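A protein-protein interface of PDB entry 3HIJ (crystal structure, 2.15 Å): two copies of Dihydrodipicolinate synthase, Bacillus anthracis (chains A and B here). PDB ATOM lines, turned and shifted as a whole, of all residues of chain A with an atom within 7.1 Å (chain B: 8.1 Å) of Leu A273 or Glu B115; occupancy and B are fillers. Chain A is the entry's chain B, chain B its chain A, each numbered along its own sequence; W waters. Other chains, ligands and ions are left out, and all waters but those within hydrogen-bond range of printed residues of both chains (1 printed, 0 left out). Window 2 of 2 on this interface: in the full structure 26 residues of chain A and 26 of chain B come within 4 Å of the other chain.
The backbone carbonyl oxygen of Pro A249 is in hydrogen-bond range of the side-chain hydroxyl of Thr A252, 3.4 Å away.
The side-chain carboxylate (OE2) of Glu B115 is in hydrogen-bond range of the side-chain amide nitrogen (NE2) of Gln B119, 2.6 Å away.
OG1 of Thr A252 sits close to O of Leu A273 (3.3 Å).
The side-chain carboxylate of Glu B115 is in salt-bridge range of the guanidinium group of Arg B152 (2.8 Å).
The side-chain hydroxyl of Ser B113 is in hydrogen-bond range of the backbone NH of Gly B116, 3.0 Å away.
N of Glu B115 lies close to OG of Ser B113 (3.5 Å).
Pro A249 touches Pro B112 (CG to C, 3.95 Å).
Pro A249 touches Ser B113 (CG to N, 3.6 Å).
Leu A270 touches Gln B119 (CD2 to CB, 3.9 Å).
Pro A271 touches Gly B116 (O to CA, 3.4 Å).
Pro A271 touches His B120 (CB to CB, 3.8 Å).
Leu A273 touches Glu B115.
CD1 of Leu A273 touches N of Gly B116 (3.7 Å).
Leu A273 touches Gln B119 (CD1 to CG, 3.9 Å).
Leu A273 touches just these residues of chain B: Glu B115, Gly B116 and Gln B119.
Glu B115 touches one residue of chain A.
No residue of chain B comes within 4 Å of Pro A274.
Printed residues of chain B within 4 Å of Leu A270: Gln B119.
Printed residues of chain A within 4 Å of Ser B113: Pro A249.
Of the printed residues of chain A, Gly B116 touches Pro A271 (3.4 Å) and Leu A273 (3.7 Å).
Printed residues of chain A within 4 Å of His B120: Pro A271 (3.8 Å).
Of the printed residues of chain A, Gln B119 touches Leu A270 (3.9 Å) and Leu A273 (3.9 Å).
The nearest residue of chain B that does not touch Leu A273 is Ser B113 (5.0 Å).
The nearest printed residue of chain B that does not touch Pro A249 is Gln B114 (6.6 Å).
Of the 16 printed residues of chain A, 4 touch a printed residue of chain B.
Hydrophobic or aromatic side chains of chain A that line the printed part of chain B: Pro A249, Leu A270, Pro A271 and Leu A273.
Among the printed residues, 8 pairs touch across the chains.
No position is printed for both chains.
Of the 8 pairs that touch across the chains among the printed residues, none has its exchanged pair printed and touching as well.
Water W1 bridges O of Pro A271 (2.8 Å) and N of Ser B113 (2.8 Å).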
ATOM      1  N   ALA A 248     -15.719  -4.822  14.954  1.00  0.00           N
ATOM      2  CA  ALA A 248     -16.209  -5.277  16.239  1.00  0.00           C
ATOM      3  C   ALA A 248     -15.135  -6.266  16.694  1.00  0.00           C
ATOM      4  O   ALA A 248     -14.351  -6.729  15.882  1.00  0.00           O
ATOM      5  CB  ALA A 248     -17.591  -5.916  16.108  1.00  0.00           C
ATOM      6  N   PRO A 249     -15.070  -6.581  17.983  1.00  0.00           N
ATOM      7  CA  PRO A 249     -13.979  -7.435  18.462  1.00  0.00           C
ATOM      8  C   PRO A 249     -13.827  -8.774  17.637  1.00  0.00           C
ATOM      9  O   PRO A 249     -14.778  -9.532  17.517  1.00  0.00           O
ATOM     10  CB  PRO A 249     -14.418  -7.745  19.906  1.00  0.00           C
ATOM     11  CG  PRO A 249     -15.169  -6.538  20.308  1.00  0.00           C
ATOM     12  CD  PRO A 249     -15.991  -6.205  19.071  1.00  0.00           C
ATOM     13  N   THR A 252     -15.537 -12.173  15.847  1.00  0.00           N
ATOM     14  CA  THR A 252     -16.956 -12.239  15.484  1.00  0.00           C
ATOM     15  C   THR A 252     -17.232 -11.814  14.022  1.00  0.00           C
ATOM     16  O   THR A 252     -17.977 -12.512  13.328  1.00  0.00           O
ATOM     17  CB  THR A 252     -17.865 -11.452  16.460  1.00  0.00           C
ATOM     18  OG1 THR A 252     -17.401 -11.689  17.773  1.00  0.00           O
ATOM     19  CG2 THR A 252     -19.340 -11.933  16.368  1.00  0.00           C
ATOM     20  N   PRO A 253     -16.616 -10.706  13.548  1.00  0.00           N
ATOM     21  CA  PRO A 253     -16.894 -10.324  12.166  1.00  0.00           C
ATOM     22  C   PRO A 253     -16.485 -11.404  11.126  1.00  0.00           C
ATOM     23  O   PRO A 253     -17.268 -11.657  10.214  1.00  0.00           O
ATOM     24  CB  PRO A 253     -16.044  -9.072  11.966  1.00  0.00           C
ATOM     25  CG  PRO A 253     -15.875  -8.504  13.314  1.00  0.00           C
ATOM     26  CD  PRO A 253     -15.705  -9.732  14.198  1.00  0.00           C
ATOM     27  N   THR A 256     -18.853 -14.186  11.153  1.00  0.00           N
ATOM     28  CA  THR A 256     -20.107 -13.795  10.511  1.00  0.00           C
ATOM     29  C   THR A 256     -19.918 -13.756   8.986  1.00  0.00           C
ATOM     30  O   THR A 256     -20.820 -14.093   8.235  1.00  0.00           O
ATOM     31  CB  THR A 256     -20.569 -12.420  11.041  1.00  0.00           C
ATOM     32  OG1 THR A 256     -20.635 -12.468  12.483  1.00  0.00           O
ATOM     33  CG2 THR A 256     -21.944 -12.027  10.427  1.00  0.00           C
ATOM     34  N   SER A 267     -21.087 -19.012  16.476  1.00  0.00           N
ATOM     35  CA  SER A 267     -20.899 -17.646  16.994  1.00  0.00           C
ATOM     36  C   SER A 267     -19.642 -17.687  17.903  1.00  0.00           C
ATOM     37  O   SER A 267     -18.742 -18.536  17.681  1.00  0.00           O
ATOM     38  CB  SER A 267     -22.185 -17.193  17.743  1.00  0.00           C
ATOM     39  OG  SER A 267     -22.001 -15.852  18.161  1.00  0.00           O
ATOM     40  N   VAL A 268     -19.634 -16.877  18.965  1.00  0.00           N
ATOM     41  CA  VAL A 268     -18.416 -16.660  19.758  1.00  0.00           C
ATOM     42  C   VAL A 268     -18.821 -16.842  21.198  1.00  0.00           C
ATOM     43  O   VAL A 268     -20.024 -16.781  21.504  1.00  0.00           O
ATOM     44  CB  VAL A 268     -17.871 -15.214  19.570  1.00  0.00           C
ATOM     45  CG1 VAL A 268     -17.212 -15.039  18.121  1.00  0.00           C
ATOM     46  CG2 VAL A 268     -19.005 -14.165  19.772  1.00  0.00           C
ATOM     47  N   ARG A 269     -17.825 -17.024  22.073  1.00  0.00           N
ATOM     48  CA  ARG A 269     -18.035 -17.147  23.499  1.00  0.00           C
ATOM     49  C   ARG A 269     -17.821 -15.807  24.191  1.00  0.00           C
ATOM     50  O   ARG A 269     -16.939 -15.000  23.782  1.00  0.00           O
ATOM     51  CB  ARG A 269     -17.064 -18.197  24.071  1.00  0.00           C
ATOM     52  CG  ARG A 269     -17.371 -19.642  23.535  1.00  0.00           C
ATOM     53  CD  ARG A 269     -16.326 -20.611  23.989  1.00  0.00           C
ATOM     54  NE  ARG A 269     -16.658 -21.992  23.661  1.00  0.00           N
ATOM     55  CZ  ARG A 269     -15.960 -23.048  24.079  1.00  0.00           C
ATOM     56  NH1 ARG A 269     -14.888 -22.887  24.856  1.00  0.00           N
ATOM     57  NH2 ARG A 269     -16.321 -24.263  23.691  1.00  0.00           N
ATOM     58  N   LEU A 270     -18.625 -15.581  25.243  1.00  0.00           N
ATOM     59  CA  LEU A 270     -18.478 -14.411  26.142  1.00  0.00           C
ATOM     60  C   LEU A 270     -17.043 -14.387  26.682  1.00  0.00           C
ATOM     61  O   LEU A 270     -16.566 -15.406  27.177  1.00  0.00           O
ATOM     62  CB  LEU A 270     -19.491 -14.498  27.288  1.00  0.00           C
ATOM     63  CG  LEU A 270     -20.926 -14.189  26.851  1.00  0.00           C
ATOM     64  CD1 LEU A 270     -21.902 -14.650  27.983  1.00  0.00           C
ATOM     65  CD2 LEU A 270     -21.138 -12.655  26.605  1.00  0.00           C
ATOM     66  N   PRO A 271     -16.381 -13.209  26.671  1.00  0.00           N
ATOM     67  CA  PRO A 271     -17.024 -11.870  26.617  1.00  0.00           C
ATOM     68  C   PRO A 271     -17.260 -11.290  25.198  1.00  0.00           C
ATOM     69  O   PRO A 271     -17.733 -10.164  25.098  1.00  0.00           O
ATOM     70  CB  PRO A 271     -16.081 -11.006  27.452  1.00  0.00           C
ATOM     71  CG  PRO A 271     -14.726 -11.580  27.048  1.00  0.00           C
ATOM     72  CD  PRO A 271     -14.988 -13.108  27.135  1.00  0.00           C
ATOM     73  N   LEU A 272     -17.021 -12.069  24.133  1.00  0.00           N
ATOM     74  CA  LEU A 272     -17.414 -11.615  22.785  1.00  0.00           C
ATOM     75  C   LEU A 272     -18.919 -11.874  22.534  1.00  0.00           C
ATOM     76  O   LEU A 272     -19.489 -12.827  23.099  1.00  0.00           O
ATOM     77  CB  LEU A 272     -16.565 -12.290  21.699  1.00  0.00           C
ATOM     78  CG  LEU A 272     -15.073 -12.210  22.011  1.00  0.00           C
ATOM     79  CD1 LEU A 272     -14.244 -12.767  20.856  1.00  0.00           C
ATOM     80  CD2 LEU A 272     -14.656 -10.729  22.372  1.00  0.00           C
ATOM     81  N   LEU A 273     -19.514 -11.065  21.659  1.00  0.00           N
ATOM     82  CA  LEU A 273     -20.936 -11.105  21.366  1.00  0.00           C
ATOM     83  C   LEU A 273     -21.167 -11.170  19.854  1.00  0.00           C
ATOM     84  O   LEU A 273     -20.302 -10.777  19.085  1.00  0.00           O
ATOM     85  CB  LEU A 273     -21.582  -9.800  21.883  1.00  0.00           C
ATOM     86  CG  LEU A 273     -21.811  -9.726  23.398  1.00  0.00           C
ATOM     87  CD1 LEU A 273     -22.496  -8.368  23.698  1.00  0.00           C
ATOM     88  CD2 LEU A 273     -22.675 -10.834  23.898  1.00  0.00           C
ATOM     89  N   PRO A 274     -22.342 -11.686  19.414  1.00  0.00           N
ATOM     90  CA  PRO A 274     -22.690 -11.655  17.993  1.00  0.00           C
ATOM     91  C   PRO A 274     -22.772 -10.232  17.524  1.00  0.00           C
ATOM     92  O   PRO A 274     -23.052  -9.317  18.315  1.00  0.00           O
ATOM     93  CB  PRO A 274     -24.086 -12.270  17.946  1.00  0.00           C
ATOM     94  CG  PRO A 274     -24.155 -13.139  19.141  1.00  0.00           C
ATOM     95  CD  PRO A 274     -23.280 -12.504  20.217  1.00  0.00           C
ATOM     96  N   LEU A 275     -22.497 -10.027  16.254  1.00  0.00           N
ATOM     97  CA  LEU A 275     -22.711  -8.710  15.628  1.00  0.00           C
ATOM     98  C   LEU A 275     -24.151  -8.240  15.850  1.00  0.00           C
ATOM     99  O   LEU A 275     -25.044  -9.049  15.855  1.00  0.00           O
ATOM    100  CB  LEU A 275     -22.507  -8.829  14.112  1.00  0.00           C
ATOM    101  CG  LEU A 275     -21.184  -8.352  13.506  1.00  0.00           C
ATOM    102  CD1 LEU A 275     -19.958  -8.546  14.347  1.00  0.00           C
ATOM    103  CD2 LEU A 275     -20.995  -8.803  12.004  1.00  0.00           C
ATOM    104  N   THR A 276     -24.374  -6.957  16.080  1.00  0.00           N
ATOM    105  CA  THR A 276     -25.777  -6.439  16.084  1.00  0.00           C
ATOM    106  C   THR A 276     -26.281  -6.465  14.629  1.00  0.00           C
ATOM    107  O   THR A 276     -25.480  -6.569  13.656  1.00  0.00           O
ATOM    108  CB  THR A 276     -25.842  -5.011  16.547  1.00  0.00           C
ATOM    109  OG1 THR A 276     -25.022  -4.215  15.697  1.00  0.00           O
ATOM    110  CG2 THR A 276     -25.303  -4.878  17.966  1.00  0.00           C
ATOM    111  N   GLU A 279     -24.542  -3.938  12.571  1.00  0.00           N
ATOM    112  CA  GLU A 279     -23.178  -4.357  12.213  1.00  0.00           C
ATOM    113  C   GLU A 279     -23.248  -5.363  11.074  1.00  0.00           C
ATOM    114  O   GLU A 279     -22.385  -5.364  10.206  1.00  0.00           O
ATOM    115  CB  GLU A 279     -22.415  -4.943  13.427  1.00  0.00           C
ATOM    116  CG  GLU A 279     -22.089  -3.880  14.457  1.00  0.00           C
ATOM    117  CD  GLU A 279     -21.590  -4.458  15.800  1.00  0.00           C
ATOM    118  OE1 GLU A 279     -22.049  -5.538  16.195  1.00  0.00           O
ATOM    119  OE2 GLU A 279     -20.742  -3.818  16.457  1.00  0.00           O
ATOM    120  N   PRO B 112     -12.797  -7.047  24.467  1.00  0.00           N
ATOM    121  CA  PRO B 112     -14.269  -6.994  24.333  1.00  0.00           C
ATOM    122  C   PRO B 112     -14.768  -5.578  24.119  1.00  0.00           C
ATOM    123  O   PRO B 112     -14.044  -4.618  24.433  1.00  0.00           O
ATOM    124  CB  PRO B 112     -14.783  -7.501  25.682  1.00  0.00           C
ATOM    125  CG  PRO B 112     -13.610  -7.181  26.719  1.00  0.00           C
ATOM    126  CD  PRO B 112     -12.336  -7.351  25.834  1.00  0.00           C
ATOM    127  N   SER B 113     -16.003  -5.425  23.608  1.00  0.00           N
ATOM    128  CA  SER B 113     -16.583  -4.108  23.419  1.00  0.00           C
ATOM    129  C   SER B 113     -17.174  -3.716  24.809  1.00  0.00           C
ATOM    130  O   SER B 113     -17.224  -4.552  25.718  1.00  0.00           O
ATOM    131  CB  SER B 113     -17.766  -4.172  22.405  1.00  0.00           C
ATOM    132  OG  SER B 113     -18.715  -5.141  22.892  1.00  0.00           O
ATOM    133  N   GLN B 114     -17.725  -2.492  24.915  1.00  0.00           N
ATOM    134  CA  GLN B 114     -18.502  -2.066  26.102  1.00  0.00           C
ATOM    135  C   GLN B 114     -19.694  -2.998  26.369  1.00  0.00           C
ATOM    136  O   GLN B 114     -19.933  -3.389  27.497  1.00  0.00           O
ATOM    137  CB  GLN B 114     -19.027  -0.624  25.880  1.00  0.00           C
ATOM    138  CG  GLN B 114     -17.864   0.418  25.770  1.00  0.00           C
ATOM    139  CD  GLN B 114     -16.921   0.344  26.983  1.00  0.00           C
ATOM    140  OE1 GLN B 114     -17.368   0.355  28.168  1.00  0.00           O
ATOM    141  NE2 GLN B 114     -15.629   0.293  26.713  1.00  0.00           N
ATOM    142  N   GLU B 115     -20.446  -3.353  25.330  1.00  0.00           N
ATOM    143  CA  GLU B 115     -21.655  -4.222  25.532  1.00  0.00           C
ATOM    144  C   GLU B 115     -21.204  -5.626  25.935  1.00  0.00           C
ATOM    145  O   GLU B 115     -21.816  -6.270  26.752  1.00  0.00           O
ATOM    146  CB  GLU B 115     -22.585  -4.229  24.294  1.00  0.00           C
ATOM    147  CG  GLU B 115     -23.841  -5.135  24.426  1.00  0.00           C
ATOM    148  CD  GLU B 115     -24.755  -4.772  25.646  1.00  0.00           C
ATOM    149  OE1 GLU B 115     -24.684  -3.653  26.121  1.00  0.00           O
ATOM    150  OE2 GLU B 115     -25.532  -5.610  26.146  1.00  0.00           O
ATOM    151  N   GLY B 116     -20.109  -6.076  25.346  1.00  0.00           N
ATOM    152  CA  GLY B 116     -19.508  -7.339  25.710  1.00  0.00           C
ATOM    153  C   GLY B 116     -19.121  -7.377  27.168  1.00  0.00           C
ATOM    154  O   GLY B 116     -19.381  -8.371  27.858  1.00  0.00           O
ATOM    155  N   MET B 117     -18.476  -6.316  27.647  1.00  0.00           N
ATOM    156  CA  MET B 117     -18.085  -6.231  29.061  1.00  0.00           C
ATOM    157  C   MET B 117     -19.321  -6.167  29.912  1.00  0.00           C
ATOM    158  O   MET B 117     -19.421  -6.817  30.933  1.00  0.00           O
ATOM    159  CB  MET B 117     -17.148  -5.029  29.306  1.00  0.00           C
ATOM    160  CG  MET B 117     -15.676  -5.394  28.908  1.00  0.00           C
ATOM    161  SD  MET B 117     -14.482  -4.113  29.248  1.00  0.00           S
ATOM    162  CE  MET B 117     -14.879  -2.885  28.017  1.00  0.00           C
ATOM    163  N   TYR B 118     -20.298  -5.393  29.457  1.00  0.00           N
ATOM    164  CA  TYR B 118     -21.546  -5.291  30.221  1.00  0.00           C
ATOM    165  C   TYR B 118     -22.129  -6.711  30.425  1.00  0.00           C
ATOM    166  O   TYR B 118     -22.436  -7.101  31.572  1.00  0.00           O
ATOM    167  CB  TYR B 118     -22.550  -4.309  29.544  1.00  0.00           C
ATOM    168  CG  TYR B 118     -23.906  -4.334  30.287  1.00  0.00           C
ATOM    169  CD1 TYR B 118     -24.070  -3.611  31.497  1.00  0.00           C
ATOM    170  CD2 TYR B 118     -24.980  -5.104  29.819  1.00  0.00           C
ATOM    171  CE1 TYR B 118     -25.255  -3.644  32.214  1.00  0.00           C
ATOM    172  CE2 TYR B 118     -26.227  -5.134  30.535  1.00  0.00           C
ATOM    173  CZ  TYR B 118     -26.327  -4.386  31.737  1.00  0.00           C
ATOM    174  OH  TYR B 118     -27.451  -4.383  32.481  1.00  0.00           O
ATOM    175  N   GLN B 119     -22.242  -7.500  29.336  1.00  0.00           N
ATOM    176  CA  GLN B 119     -22.812  -8.869  29.440  1.00  0.00           C
ATOM    177  C   GLN B 119     -21.887  -9.761  30.324  1.00  0.00           C
ATOM    178  O   GLN B 119     -22.336 -10.580  31.113  1.00  0.00           O
ATOM    179  CB  GLN B 119     -23.027  -9.504  28.031  1.00  0.00           C
ATOM    180  CG  GLN B 119     -24.083  -8.686  27.192  1.00  0.00           C
ATOM    181  CD  GLN B 119     -25.436  -8.655  27.872  1.00  0.00           C
ATOM    182  OE1 GLN B 119     -25.762  -9.569  28.661  1.00  0.00           O
ATOM    183  NE2 GLN B 119     -26.251  -7.606  27.565  1.00  0.00           N
ATOM    184  N   HIS B 120     -20.592  -9.556  30.203  1.00  0.00           N
ATOM    185  CA  HIS B 120     -19.609 -10.398  30.921  1.00  0.00           C
ATOM    186  C   HIS B 120     -19.843 -10.146  32.440  1.00  0.00           C
ATOM    187  O   HIS B 120     -20.137 -11.056  33.192  1.00  0.00           O
ATOM    188  CB  HIS B 120     -18.186  -9.952  30.469  1.00  0.00           C
ATOM    189  CG  HIS B 120     -17.052 -10.407  31.361  1.00  0.00           C
ATOM    190  ND1 HIS B 120     -16.440 -11.633  31.212  1.00  0.00           N
ATOM    191  CD2 HIS B 120     -16.398  -9.789  32.387  1.00  0.00           C
ATOM    192  CE1 HIS B 120     -15.455 -11.750  32.097  1.00  0.00           C
ATOM    193  NE2 HIS B 120     -15.399 -10.636  32.814  1.00  0.00           N
ATOM    194  N   PHE B 121     -19.733  -8.897  32.875  1.00  0.00           N
ATOM    195  CA  PHE B 121     -19.861  -8.585  34.311  1.00  0.00           C
ATOM    196  C   PHE B 121     -21.252  -8.930  34.834  1.00  0.00           C
ATOM    197  O   PHE B 121     -21.369  -9.445  35.946  1.00  0.00           O
ATOM    198  CB  PHE B 121     -19.538  -7.113  34.527  1.00  0.00           C
ATOM    199  CG  PHE B 121     -18.090  -6.775  34.269  1.00  0.00           C
ATOM    200  CD1 PHE B 121     -17.087  -7.366  35.041  1.00  0.00           C
ATOM    201  CD2 PHE B 121     -17.738  -5.799  33.362  1.00  0.00           C
ATOM    202  CE1 PHE B 121     -15.738  -7.012  34.863  1.00  0.00           C
ATOM    203  CE2 PHE B 121     -16.410  -5.450  33.168  1.00  0.00           C
ATOM    204  CZ  PHE B 121     -15.410  -6.066  33.961  1.00  0.00           C
ATOM    205  N   LYS B 122     -22.293  -8.652  34.033  1.00  0.00           N
ATOM    206  CA  LYS B 122     -23.677  -8.970  34.393  1.00  0.00           C
ATOM    207  C   LYS B 122     -23.833 -10.443  34.645  1.00  0.00           C
ATOM    208  O   LYS B 122     -24.360 -10.851  35.705  1.00  0.00           O
ATOM    209  CB  LYS B 122     -24.660  -8.489  33.291  1.00  0.00           C
ATOM    210  CG  LYS B 122     -26.181  -8.842  33.534  1.00  0.00           C
ATOM    211  CD  LYS B 122     -27.080  -8.139  32.463  1.00  0.00           C
ATOM    212  CE  LYS B 122     -28.587  -8.447  32.521  1.00  0.00           C
ATOM    213  NZ  LYS B 122     -28.913  -9.900  32.608  1.00  0.00           N
ATOM    214  N   SER B 146     -16.038   1.946  30.121  1.00  0.00           N
ATOM    215  CA  SER B 146     -16.490   3.320  29.995  1.00  0.00           C
ATOM    216  C   SER B 146     -17.307   3.745  31.211  1.00  0.00           C
ATOM    217  O   SER B 146     -17.943   2.917  31.896  1.00  0.00           O
ATOM    218  CB  SER B 146     -17.325   3.551  28.707  1.00  0.00           C
ATOM    219  OG  SER B 146     -18.605   2.973  28.899  1.00  0.00           O
ATOM    220  N   THR B 149     -20.749   2.417  30.843  1.00  0.00           N
ATOM    221  CA  THR B 149     -20.800   1.002  31.188  1.00  0.00           C
ATOM    222  C   THR B 149     -20.765   0.767  32.707  1.00  0.00           C
ATOM    223  O   THR B 149     -21.536  -0.054  33.249  1.00  0.00           O
ATOM    224  CB  THR B 149     -19.681   0.205  30.455  1.00  0.00           C
ATOM    225  OG1 THR B 149     -19.839   0.410  29.062  1.00  0.00           O
ATOM    226  CG2 THR B 149     -19.824  -1.233  30.671  1.00  0.00           C
ATOM    227  N   ARG B 152     -24.216   1.726  34.160  1.00  0.00           N
ATOM    228  CA  ARG B 152     -25.181   0.649  33.933  1.00  0.00           C
ATOM    229  C   ARG B 152     -24.963  -0.519  34.862  1.00  0.00           C
ATOM    230  O   ARG B 152     -25.919  -1.086  35.389  1.00  0.00           O
ATOM    231  CB  ARG B 152     -25.082   0.112  32.485  1.00  0.00           C
ATOM    232  CG  ARG B 152     -25.482   1.107  31.383  1.00  0.00           C
ATOM    233  CD  ARG B 152     -25.266   0.449  30.035  1.00  0.00           C
ATOM    234  NE  ARG B 152     -26.240  -0.634  29.811  1.00  0.00           N
ATOM    235  CZ  ARG B 152     -26.157  -1.573  28.858  1.00  0.00           C
ATOM    236  NH1 ARG B 152     -25.096  -1.645  28.080  1.00  0.00           N
ATOM    237  NH2 ARG B 152     -27.143  -2.459  28.709  1.00  0.00           N
ATOM    238  N   LEU B 153     -23.701  -0.957  35.008  1.00  0.00           N
ATOM    239  CA  LEU B 153     -23.438  -2.055  35.920  1.00  0.00           C
ATOM    240  C   LEU B 153     -23.749  -1.725  37.411  1.00  0.00           C
ATOM    241  O   LEU B 153     -24.136  -2.620  38.194  1.00  0.00           O
ATOM    242  CB  LEU B 153     -21.975  -2.534  35.747  1.00  0.00           C
ATOM    243  CG  LEU B 153     -21.716  -3.215  34.399  1.00  0.00           C
ATOM    244  CD1 LEU B 153     -20.246  -3.184  34.029  1.00  0.00           C
ATOM    245  CD2 LEU B 153     -22.371  -4.673  34.377  1.00  0.00           C
HETATM  246  O   HOH W   1     -17.157  -7.999  23.434  1.00  0.00           O
